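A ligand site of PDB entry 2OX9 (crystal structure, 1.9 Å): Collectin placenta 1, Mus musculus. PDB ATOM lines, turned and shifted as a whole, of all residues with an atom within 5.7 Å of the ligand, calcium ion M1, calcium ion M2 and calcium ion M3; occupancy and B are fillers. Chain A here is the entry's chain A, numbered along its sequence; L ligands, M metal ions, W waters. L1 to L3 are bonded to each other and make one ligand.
An oxygen (O3) of LIG L1 is in hydrogen-bond range of the side-chain amino group (NZ) of Lys 89, at 2.9 Å.
The backbone NH (N) of Asn 95 is in hydrogen-bond range of the side-chain carboxylate (OD2) of Asp 117, at 2.7 Å. OE1 of Glu 104 sits close to N of Trp 96. The backbone NH (N) of Asp 105 sits at hydrogen-bond distance from the backbone carbonyl oxygen (O) of Phe 118 (3.3 Å). The backbone NH of Ser 73 sits close to the side-chain carboxylate of Asp 68 (2.9 Å). The side-chain carboxylate (OD1) of Asp 94 lies close to the backbone NH (N) of Trp 96, 3.4 Å away.
CE2 of Trp 96 touches O5 of LG3 L3, at 3.8 Å. Hydrophobic or aromatic side chains within 4 Å of the ligand: Trp 96. Of the 20 residues printed, 7 come within 4 Å of the ligand. Along chain A the residues within 4 Å of the ligand span positions 89 to 117. The nearest printed residue that does not touch the ligand is Ile 110 (4.1 Å).
Within 4 Å of calcium ion M2: Gln 92, Asp 94, Glu 104, Asn 116 and Asp 117. The nearest printed residue that does not touch calcium ion M2 is Phe 118 (4.7 Å).
Of the 20 residues printed, 4 come within 4 Å of calcium ion M3.
Calcium ion M1 is bound by O of Glu 104 (2.3 Å), OE2 of Glu 72 (2.4 Å), OD2 of Asp 68 (2.4 Å), OD1 of Asp 105 (2.4 Å), OD1 of Asn 95 (2.5 Å), OE1 of Glu 72 (2.6 Å), water W1 (2.6 Å) and OD1 of Asp 68 (2.7 Å).
Calcium ion M2 is bound by OD1 of Asp 117 (2.1 Å), O2 of LG3 L3 (2.3 Å), OD1 of Asn 116 (2.4 Å), OE1 of Glu 104 (2.4 Å), OE1 of Gln 92 (2.4 Å), O of Asp 117 (2.5 Å), OD1 of Asp 94 (2.5 Å) and O3 of LG3 L3 (2.7 Å).
Calcium ion M3 is bound by water W4 (2.1 Å), the side-chain carboxylate (OE1) of Glu 72 (2.3 Å), the side-chain carboxylate (OD2) of Asp 105 (2.3 Å), the backbone carbonyl oxygen (O) of Pro 102 (2.4 Å), the side-chain carboxylate (OD1) of Asp 105 (2.5 Å) and water W10 (2.5 Å).
Water W1 bridges OD2 of Asp 117 (2.7 Å) and N of Asn 95 (3.2 Å). Water W3 lies within hydrogen-bond range of O3 of LIG L1, NE2 of Gln 92 and O of Ala 90. Water W2 lies within hydrogen-bond range of O1 of LG3 L3 (2.5 Å) and ND2 of Asn 116 (3.5 Å).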
ATOM      1  N   ASP A  68       2.832 -11.199 -30.052  1.00  0.00           N
ATOM      2  CA  ASP A  68       2.723 -12.383 -30.897  1.00  0.00           C
ATOM      3  C   ASP A  68       1.261 -12.508 -31.334  1.00  0.00           C
ATOM      4  O   ASP A  68       0.719 -13.609 -31.443  1.00  0.00           O
ATOM      5  CB  ASP A  68       3.216 -13.648 -30.153  1.00  0.00           C
ATOM      6  CG  ASP A  68       2.239 -14.125 -29.091  1.00  0.00           C
ATOM      7  OD1 ASP A  68       1.464 -13.316 -28.573  1.00  0.00           O
ATOM      8  OD2 ASP A  68       2.264 -15.337 -28.768  1.00  0.00           O
ATOM      9  N   SER A  69       0.645 -11.356 -31.575  1.00  0.00           N
ATOM     10  CA  SER A  69      -0.748 -11.274 -32.017  1.00  0.00           C
ATOM     11  C   SER A  69      -0.902 -11.715 -33.467  1.00  0.00           C
ATOM     12  O   SER A  69      -1.906 -12.321 -33.823  1.00  0.00           O
ATOM     13  CB  SER A  69      -1.270  -9.845 -31.885  1.00  0.00           C
ATOM     14  OG  SER A  69      -1.293  -9.413 -30.537  1.00  0.00           O
ATOM     15  N   GLU A  72       0.461 -16.570 -33.057  1.00  0.00           N
ATOM     16  CA  GLU A  72       0.780 -17.097 -31.737  1.00  0.00           C
ATOM     17  C   GLU A  72       2.172 -17.743 -31.686  1.00  0.00           C
ATOM     18  O   GLU A  72       2.532 -18.531 -32.565  1.00  0.00           O
ATOM     19  CB  GLU A  72      -0.294 -18.097 -31.306  1.00  0.00           C
ATOM     20  CG  GLU A  72      -0.166 -18.640 -29.890  1.00  0.00           C
ATOM     21  CD  GLU A  72      -0.152 -17.543 -28.836  1.00  0.00           C
ATOM     22  OE1 GLU A  72      -0.906 -16.563 -29.000  1.00  0.00           O
ATOM     23  OE2 GLU A  72       0.591 -17.665 -27.852  1.00  0.00           O
ATOM     24  N   SER A  73       2.937 -17.391 -30.658  1.00  0.00           N
ATOM     25  CA  SER A  73       4.288 -17.900 -30.427  1.00  0.00           C
ATOM     26  C   SER A  73       5.383 -17.309 -31.291  1.00  0.00           C
ATOM     27  O   SER A  73       6.558 -17.612 -31.108  1.00  0.00           O
ATOM     28  CB  SER A  73       4.323 -19.429 -30.533  1.00  0.00           C
ATOM     29  OG  SER A  73       3.680 -20.017 -29.416  1.00  0.00           O
ATOM     30  N   TRP A  75       6.989 -14.167 -31.689  1.00  0.00           N
ATOM     31  CA  TRP A  75       7.200 -12.860 -31.087  1.00  0.00           C
ATOM     32  C   TRP A  75       8.062 -11.913 -31.911  1.00  0.00           C
ATOM     33  O   TRP A  75       9.146 -12.283 -32.342  1.00  0.00           O
ATOM     34  CB  TRP A  75       7.788 -13.021 -29.679  1.00  0.00           C
ATOM     35  CG  TRP A  75       6.832 -13.638 -28.708  1.00  0.00           C
ATOM     36  CD1 TRP A  75       6.631 -14.975 -28.496  1.00  0.00           C
ATOM     37  CD2 TRP A  75       5.911 -12.952 -27.857  1.00  0.00           C
ATOM     38  NE1 TRP A  75       5.643 -15.149 -27.557  1.00  0.00           N
ATOM     39  CE2 TRP A  75       5.183 -13.925 -27.149  1.00  0.00           C
ATOM     40  CE3 TRP A  75       5.628 -11.591 -27.629  1.00  0.00           C
ATOM     41  CZ2 TRP A  75       4.193 -13.597 -26.218  1.00  0.00           C
ATOM     42  CZ3 TRP A  75       4.645 -11.269 -26.702  1.00  0.00           C
ATOM     43  CH2 TRP A  75       3.930 -12.265 -26.014  1.00  0.00           C
ATOM     44  N   LYS A  89      10.930 -14.966 -18.272  1.00  0.00           N
ATOM     45  CA  LYS A  89      11.095 -15.624 -16.999  1.00  0.00           C
ATOM     46  C   LYS A  89      10.876 -17.098 -17.354  1.00  0.00           C
ATOM     47  O   LYS A  89      10.171 -17.402 -18.318  1.00  0.00           O
ATOM     48  CB  LYS A  89      10.008 -15.153 -16.016  1.00  0.00           C
ATOM     49  CG  LYS A  89       9.974 -15.930 -14.698  1.00  0.00           C
ATOM     50  CD  LYS A  89       8.835 -15.463 -13.824  1.00  0.00           C
ATOM     51  CE  LYS A  89       8.745 -16.271 -12.536  1.00  0.00           C
ATOM     52  NZ  LYS A  89       7.585 -15.840 -11.723  1.00  0.00           N
ATOM     53  N   ALA A  90      11.484 -18.013 -16.601  1.00  0.00           N
ATOM     54  CA  ALA A  90      11.341 -19.437 -16.889  1.00  0.00           C
ATOM     55  C   ALA A  90       9.861 -19.838 -16.836  1.00  0.00           C
ATOM     56  O   ALA A  90       9.168 -19.520 -15.877  1.00  0.00           O
ATOM     57  CB  ALA A  90      12.150 -20.255 -15.892  1.00  0.00           C
ATOM     58  N   GLN A  92       7.680 -18.837 -19.007  1.00  0.00           N
ATOM     59  CA  GLN A  92       6.992 -17.868 -19.849  1.00  0.00           C
ATOM     60  C   GLN A  92       7.645 -17.872 -21.231  1.00  0.00           C
ATOM     61  O   GLN A  92       8.815 -18.194 -21.363  1.00  0.00           O
ATOM     62  CB  GLN A  92       7.096 -16.470 -19.240  1.00  0.00           C
ATOM     63  CG  GLN A  92       6.435 -16.351 -17.900  1.00  0.00           C
ATOM     64  CD  GLN A  92       5.028 -16.910 -17.921  1.00  0.00           C
ATOM     65  OE1 GLN A  92       4.179 -16.457 -18.684  1.00  0.00           O
ATOM     66  NE2 GLN A  92       4.783 -17.912 -17.080  1.00  0.00           N
ATOM     67  N   PRO A  93       6.885 -17.515 -22.285  1.00  0.00           N
ATOM     68  CA  PRO A  93       5.470 -17.111 -22.302  1.00  0.00           C
ATOM     69  C   PRO A  93       4.556 -18.323 -22.175  1.00  0.00           C
ATOM     70  O   PRO A  93       4.832 -19.374 -22.742  1.00  0.00           O
ATOM     71  CB  PRO A  93       5.328 -16.399 -23.649  1.00  0.00           C
ATOM     72  CG  PRO A  93       6.331 -17.114 -24.511  1.00  0.00           C
ATOM     73  CD  PRO A  93       7.510 -17.272 -23.607  1.00  0.00           C
ATOM     74  N   ASP A  94       3.471 -18.191 -21.417  1.00  0.00           N
ATOM     75  CA  ASP A  94       2.571 -19.326 -21.222  1.00  0.00           C
ATOM     76  C   ASP A  94       1.211 -19.198 -21.902  1.00  0.00           C
ATOM     77  O   ASP A  94       0.419 -20.136 -21.868  1.00  0.00           O
ATOM     78  CB  ASP A  94       2.398 -19.595 -19.729  1.00  0.00           C
ATOM     79  CG  ASP A  94       1.777 -18.424 -18.985  1.00  0.00           C
ATOM     80  OD1 ASP A  94       1.594 -17.359 -19.602  1.00  0.00           O
ATOM     81  OD2 ASP A  94       1.467 -18.577 -17.782  1.00  0.00           O
ATOM     82  N   ASN A  95       0.943 -18.040 -22.501  1.00  0.00           N
ATOM     83  CA  ASN A  95      -0.325 -17.780 -23.192  1.00  0.00           C
ATOM     84  C   ASN A  95      -1.515 -18.191 -22.319  1.00  0.00           C
ATOM     85  O   ASN A  95      -2.469 -18.806 -22.791  1.00  0.00           O
ATOM     86  CB  ASN A  95      -0.345 -18.563 -24.518  1.00  0.00           C
ATOM     87  CG  ASN A  95      -1.207 -17.894 -25.581  1.00  0.00           C
ATOM     88  OD1 ASN A  95      -1.107 -16.678 -25.810  1.00  0.00           O
ATOM     89  ND2 ASN A  95      -2.043 -18.683 -26.243  1.00  0.00           N
ATOM     90  N   TRP A  96      -1.457 -17.827 -21.052  1.00  0.00           N
ATOM     91  CA  TRP A  96      -2.497 -18.153 -20.079  1.00  0.00           C
ATOM     92  C   TRP A  96      -3.891 -17.758 -20.569  1.00  0.00           C
ATOM     93  O   TRP A  96      -4.089 -16.661 -21.085  1.00  0.00           O
ATOM     94  CB  TRP A  96      -2.195 -17.449 -18.758  1.00  0.00           C
ATOM     95  CG  TRP A  96      -2.813 -18.070 -17.554  1.00  0.00           C
ATOM     96  CD1 TRP A  96      -3.772 -17.526 -16.754  1.00  0.00           C
ATOM     97  CD2 TRP A  96      -2.479 -19.344 -16.978  1.00  0.00           C
ATOM     98  NE1 TRP A  96      -4.057 -18.388 -15.710  1.00  0.00           N
ATOM     99  CE2 TRP A  96      -3.280 -19.504 -15.829  1.00  0.00           C
ATOM    100  CE3 TRP A  96      -1.588 -20.368 -17.327  1.00  0.00           C
ATOM    101  CZ2 TRP A  96      -3.203 -20.641 -15.018  1.00  0.00           C
ATOM    102  CZ3 TRP A  96      -1.515 -21.503 -16.525  1.00  0.00           C
ATOM    103  CH2 TRP A  96      -2.327 -21.621 -15.378  1.00  0.00           C
ATOM    104  N   PRO A 102      -7.922 -15.193 -26.842  1.00  0.00           N
ATOM    105  CA  PRO A 102      -6.662 -15.106 -27.579  1.00  0.00           C
ATOM    106  C   PRO A 102      -5.408 -15.350 -26.744  1.00  0.00           C
ATOM    107  O   PRO A 102      -4.291 -15.379 -27.272  1.00  0.00           O
ATOM    108  CB  PRO A 102      -6.707 -13.686 -28.154  1.00  0.00           C
ATOM    109  CG  PRO A 102      -7.403 -12.943 -27.063  1.00  0.00           C
ATOM    110  CD  PRO A 102      -8.539 -13.864 -26.672  1.00  0.00           C
ATOM    111  N   GLY A 103      -5.605 -15.512 -25.430  1.00  0.00           N
ATOM    112  CA  GLY A 103      -4.489 -15.756 -24.547  1.00  0.00           C
ATOM    113  C   GLY A 103      -3.736 -14.496 -24.159  1.00  0.00           C
ATOM    114  O   GLY A 103      -4.341 -13.462 -23.876  1.00  0.00           O
ATOM    115  N   GLU A 104      -2.411 -14.586 -24.157  1.00  0.00           N
ATOM    116  CA  GLU A 104      -1.541 -13.455 -23.806  1.00  0.00           C
ATOM    117  C   GLU A 104      -0.639 -13.199 -24.998  1.00  0.00           C
ATOM    118  O   GLU A 104       0.220 -14.020 -25.334  1.00  0.00           O
ATOM    119  CB  GLU A 104      -0.715 -13.798 -22.560  1.00  0.00           C
ATOM    120  CG  GLU A 104      -1.589 -14.161 -21.347  1.00  0.00           C
ATOM    121  CD  GLU A 104      -0.800 -14.342 -20.066  1.00  0.00           C
ATOM    122  OE1 GLU A 104       0.039 -15.264 -19.996  1.00  0.00           O
ATOM    123  OE2 GLU A 104      -1.013 -13.558 -19.117  1.00  0.00           O
ATOM    124  N   ASP A 105      -0.801 -12.042 -25.628  1.00  0.00           N
ATOM    125  CA  ASP A 105      -0.026 -11.728 -26.805  1.00  0.00           C
ATOM    126  C   ASP A 105       0.777 -10.424 -26.720  1.00  0.00           C
ATOM    127  O   ASP A 105       1.261  -9.920 -27.742  1.00  0.00           O
ATOM    128  CB  ASP A 105      -0.959 -11.660 -28.024  1.00  0.00           C
ATOM    129  CG  ASP A 105      -1.758 -12.945 -28.222  1.00  0.00           C
ATOM    130  OD1 ASP A 105      -1.472 -13.949 -27.528  1.00  0.00           O
ATOM    131  OD2 ASP A 105      -2.674 -12.937 -29.072  1.00  0.00           O
ATOM    132  N   ILE A 110       8.458  -7.708 -15.624  1.00  0.00           N
ATOM    133  CA  ILE A 110       7.966  -7.956 -14.281  1.00  0.00           C
ATOM    134  C   ILE A 110       9.132  -7.943 -13.286  1.00  0.00           C
ATOM    135  O   ILE A 110      10.108  -7.215 -13.490  1.00  0.00           O
ATOM    136  CB  ILE A 110       7.199  -9.306 -14.197  1.00  0.00           C
ATOM    137  CG1 ILE A 110       8.039 -10.415 -14.810  1.00  0.00           C
ATOM    138  CG2 ILE A 110       5.855  -9.170 -14.907  1.00  0.00           C
ATOM    139  CD1 ILE A 110       7.408 -11.789 -14.674  1.00  0.00           C
ATOM    140  N   ASN A 116       7.304 -11.299 -19.296  1.00  0.00           N
ATOM    141  CA  ASN A 116       6.128 -12.115 -19.133  1.00  0.00           C
ATOM    142  C   ASN A 116       5.102 -11.686 -20.169  1.00  0.00           C
ATOM    143  O   ASN A 116       5.058 -10.524 -20.555  1.00  0.00           O
ATOM    144  CB  ASN A 116       5.535 -11.944 -17.744  1.00  0.00           C
ATOM    145  CG  ASN A 116       4.166 -12.556 -17.632  1.00  0.00           C
ATOM    146  OD1 ASN A 116       3.976 -13.732 -17.962  1.00  0.00           O
ATOM    147  ND2 ASN A 116       3.202 -11.774 -17.168  1.00  0.00           N
ATOM    148  N   ASP A 117       4.286 -12.623 -20.630  1.00  0.00           N
ATOM    149  CA  ASP A 117       3.255 -12.295 -21.594  1.00  0.00           C
ATOM    150  C   ASP A 117       1.965 -12.034 -20.831  1.00  0.00           C
ATOM    151  O   ASP A 117       1.611 -12.784 -19.910  1.00  0.00           O
ATOM    152  CB  ASP A 117       3.090 -13.449 -22.621  1.00  0.00           C
ATOM    153  CG  ASP A 117       2.843 -14.803 -21.970  1.00  0.00           C
ATOM    154  OD1 ASP A 117       3.288 -15.027 -20.821  1.00  0.00           O
ATOM    155  OD2 ASP A 117       2.215 -15.671 -22.622  1.00  0.00           O
ATOM    156  N   PHE A 118       1.291 -10.939 -21.172  1.00  0.00           N
ATOM    157  CA  PHE A 118       0.040 -10.559 -20.520  1.00  0.00           C
ATOM    158  C   PHE A 118      -1.063 -10.481 -21.571  1.00  0.00           C
ATOM    159  O   PHE A 118      -0.795 -10.421 -22.773  1.00  0.00           O
ATOM    160  CB  PHE A 118       0.100  -9.155 -19.899  1.00  0.00           C
ATOM    161  CG  PHE A 118       1.193  -8.961 -18.884  1.00  0.00           C
ATOM    162  CD1 PHE A 118       2.486  -8.666 -19.291  1.00  0.00           C
ATOM    163  CD2 PHE A 118       0.898  -8.957 -17.527  1.00  0.00           C
ATOM    164  CE1 PHE A 118       3.475  -8.378 -18.360  1.00  0.00           C
ATOM    165  CE2 PHE A 118       1.885  -8.665 -16.584  1.00  0.00           C
ATOM    166  CZ  PHE A 118       3.180  -8.374 -17.003  1.00  0.00           C
HETATM  167  C1  LIG L   1       3.858 -15.974 -11.117  1.00  0.00           C
HETATM  168  C2  LIG L   1       4.256 -17.459 -11.201  1.00  0.00           C
HETATM  169  C3  LIG L   1       3.867 -18.023 -12.566  1.00  0.00           C
HETATM  170  C4  LIG L   1       4.477 -17.173 -13.676  1.00  0.00           C
HETATM  171  C5  LIG L   1       4.034 -15.716 -13.515  1.00  0.00           C
HETATM  172  C6  LIG L   1       4.677 -14.800 -14.556  1.00  0.00           C
HETATM  173  O1  LIG L   1       3.600 -18.192 -10.181  1.00  0.00           O
HETATM  174  O2  LIG L   1       4.316 -19.365 -12.675  1.00  0.00           O
HETATM  175  O3  LIG L   1       5.892 -17.258 -13.618  1.00  0.00           O
HETATM  176  O4  LIG L   1       4.405 -15.225 -12.204  1.00  0.00           O
HETATM  177  C1  LG2 L   2       0.854 -13.416  -8.653  1.00  0.00           C
HETATM  178  C2  LG2 L   2       1.449 -14.739  -9.127  1.00  0.00           C
HETATM  179  C3  LG2 L   2       1.984 -14.594 -10.548  1.00  0.00           C
HETATM  180  C4  LG2 L   2       0.870 -14.083 -11.463  1.00  0.00           C
HETATM  181  C5  LG2 L   2       0.293 -12.788 -10.899  1.00  0.00           C
HETATM  182  C6  LG2 L   2      -0.896 -12.292 -11.710  1.00  0.00           C
HETATM  183  C7  LG2 L   2       2.576 -16.412  -7.810  1.00  0.00           C
HETATM  184  C8  LG2 L   2       3.400 -16.683  -6.567  1.00  0.00           C
HETATM  185  N1  LG2 L   2       2.511 -15.147  -8.221  1.00  0.00           N
HETATM  186  O1  LG2 L   2       0.301 -13.586  -7.395  1.00  0.00           O
HETATM  187  O2  LG2 L   2       2.468 -15.860 -11.027  1.00  0.00           O
HETATM  188  O3  LG2 L   2       1.385 -13.857 -12.786  1.00  0.00           O
HETATM  189  O4  LG2 L   2      -0.187 -13.006  -9.548  1.00  0.00           O
HETATM  190  O5  LG2 L   2      -1.894 -13.289 -11.813  1.00  0.00           O
HETATM  191  O6  LG2 L   2       2.017 -17.346  -8.402  1.00  0.00           O
HETATM  192  C1  LG3 L   3       0.631 -14.364 -13.835  1.00  0.00           C
HETATM  193  C2  LG3 L   3       1.076 -13.695 -15.137  1.00  0.00           C
HETATM  194  C3  LG3 L   3       0.342 -14.319 -16.331  1.00  0.00           C
HETATM  195  C4  LG3 L   3       0.468 -15.840 -16.314  1.00  0.00           C
HETATM  196  C5  LG3 L   3       0.070 -16.405 -14.948  1.00  0.00           C
HETATM  197  C6  LG3 L   3       0.308 -17.904 -14.839  1.00  0.00           C
HETATM  198  O1  LG3 L   3       0.795 -12.311 -15.076  1.00  0.00           O
HETATM  199  O2  LG3 L   3       0.900 -13.803 -17.525  1.00  0.00           O
HETATM  200  O3  LG3 L   3       1.808 -16.209 -16.616  1.00  0.00           O
HETATM  201  O4  LG3 L   3       0.845 -15.779 -13.898  1.00  0.00           O
HETATM  202  O5  LG3 L   3      -0.358 -18.452 -13.717  1.00  0.00           O
HETATM  203 CA    CA M   1       0.450 -15.372 -27.179  1.00  0.00          CA
HETATM  204 CA    CA M   2       2.227 -15.022 -19.006  1.00  0.00          CA
HETATM  205 CA    CA M   3      -2.810 -15.257 -29.121  1.00  0.00          CA
HETATM  206  O   HOH W   1       1.810 -16.443 -25.192  1.00  0.00           O
HETATM  207  O   HOH W   2       2.667 -11.161 -13.783  1.00  0.00           O
HETATM  208  O   HOH W   3       6.339 -19.177 -15.098  1.00  0.00           O
HETATM  209  O   HOH W   4      -1.852 -15.056 -31.000  1.00  0.00           O
HETATM  210  O   HOH W   5       4.397 -11.861 -11.566  1.00  0.00           O
HETATM  211  O   HOH W   6       7.195 -19.988 -12.040  1.00  0.00           O
HETATM  212  O   HOH W   7       5.317 -21.552 -15.060  1.00  0.00           O
HETATM  213  O   HOH W   8       2.762 -21.797 -12.438  1.00  0.00           O
HETATM  214  O   HOH W   9      -1.459 -11.355 -15.705  1.00  0.00           O
HETATM  215  O   HOH W  10      -3.712 -17.601 -29.153  1.00  0.00           O
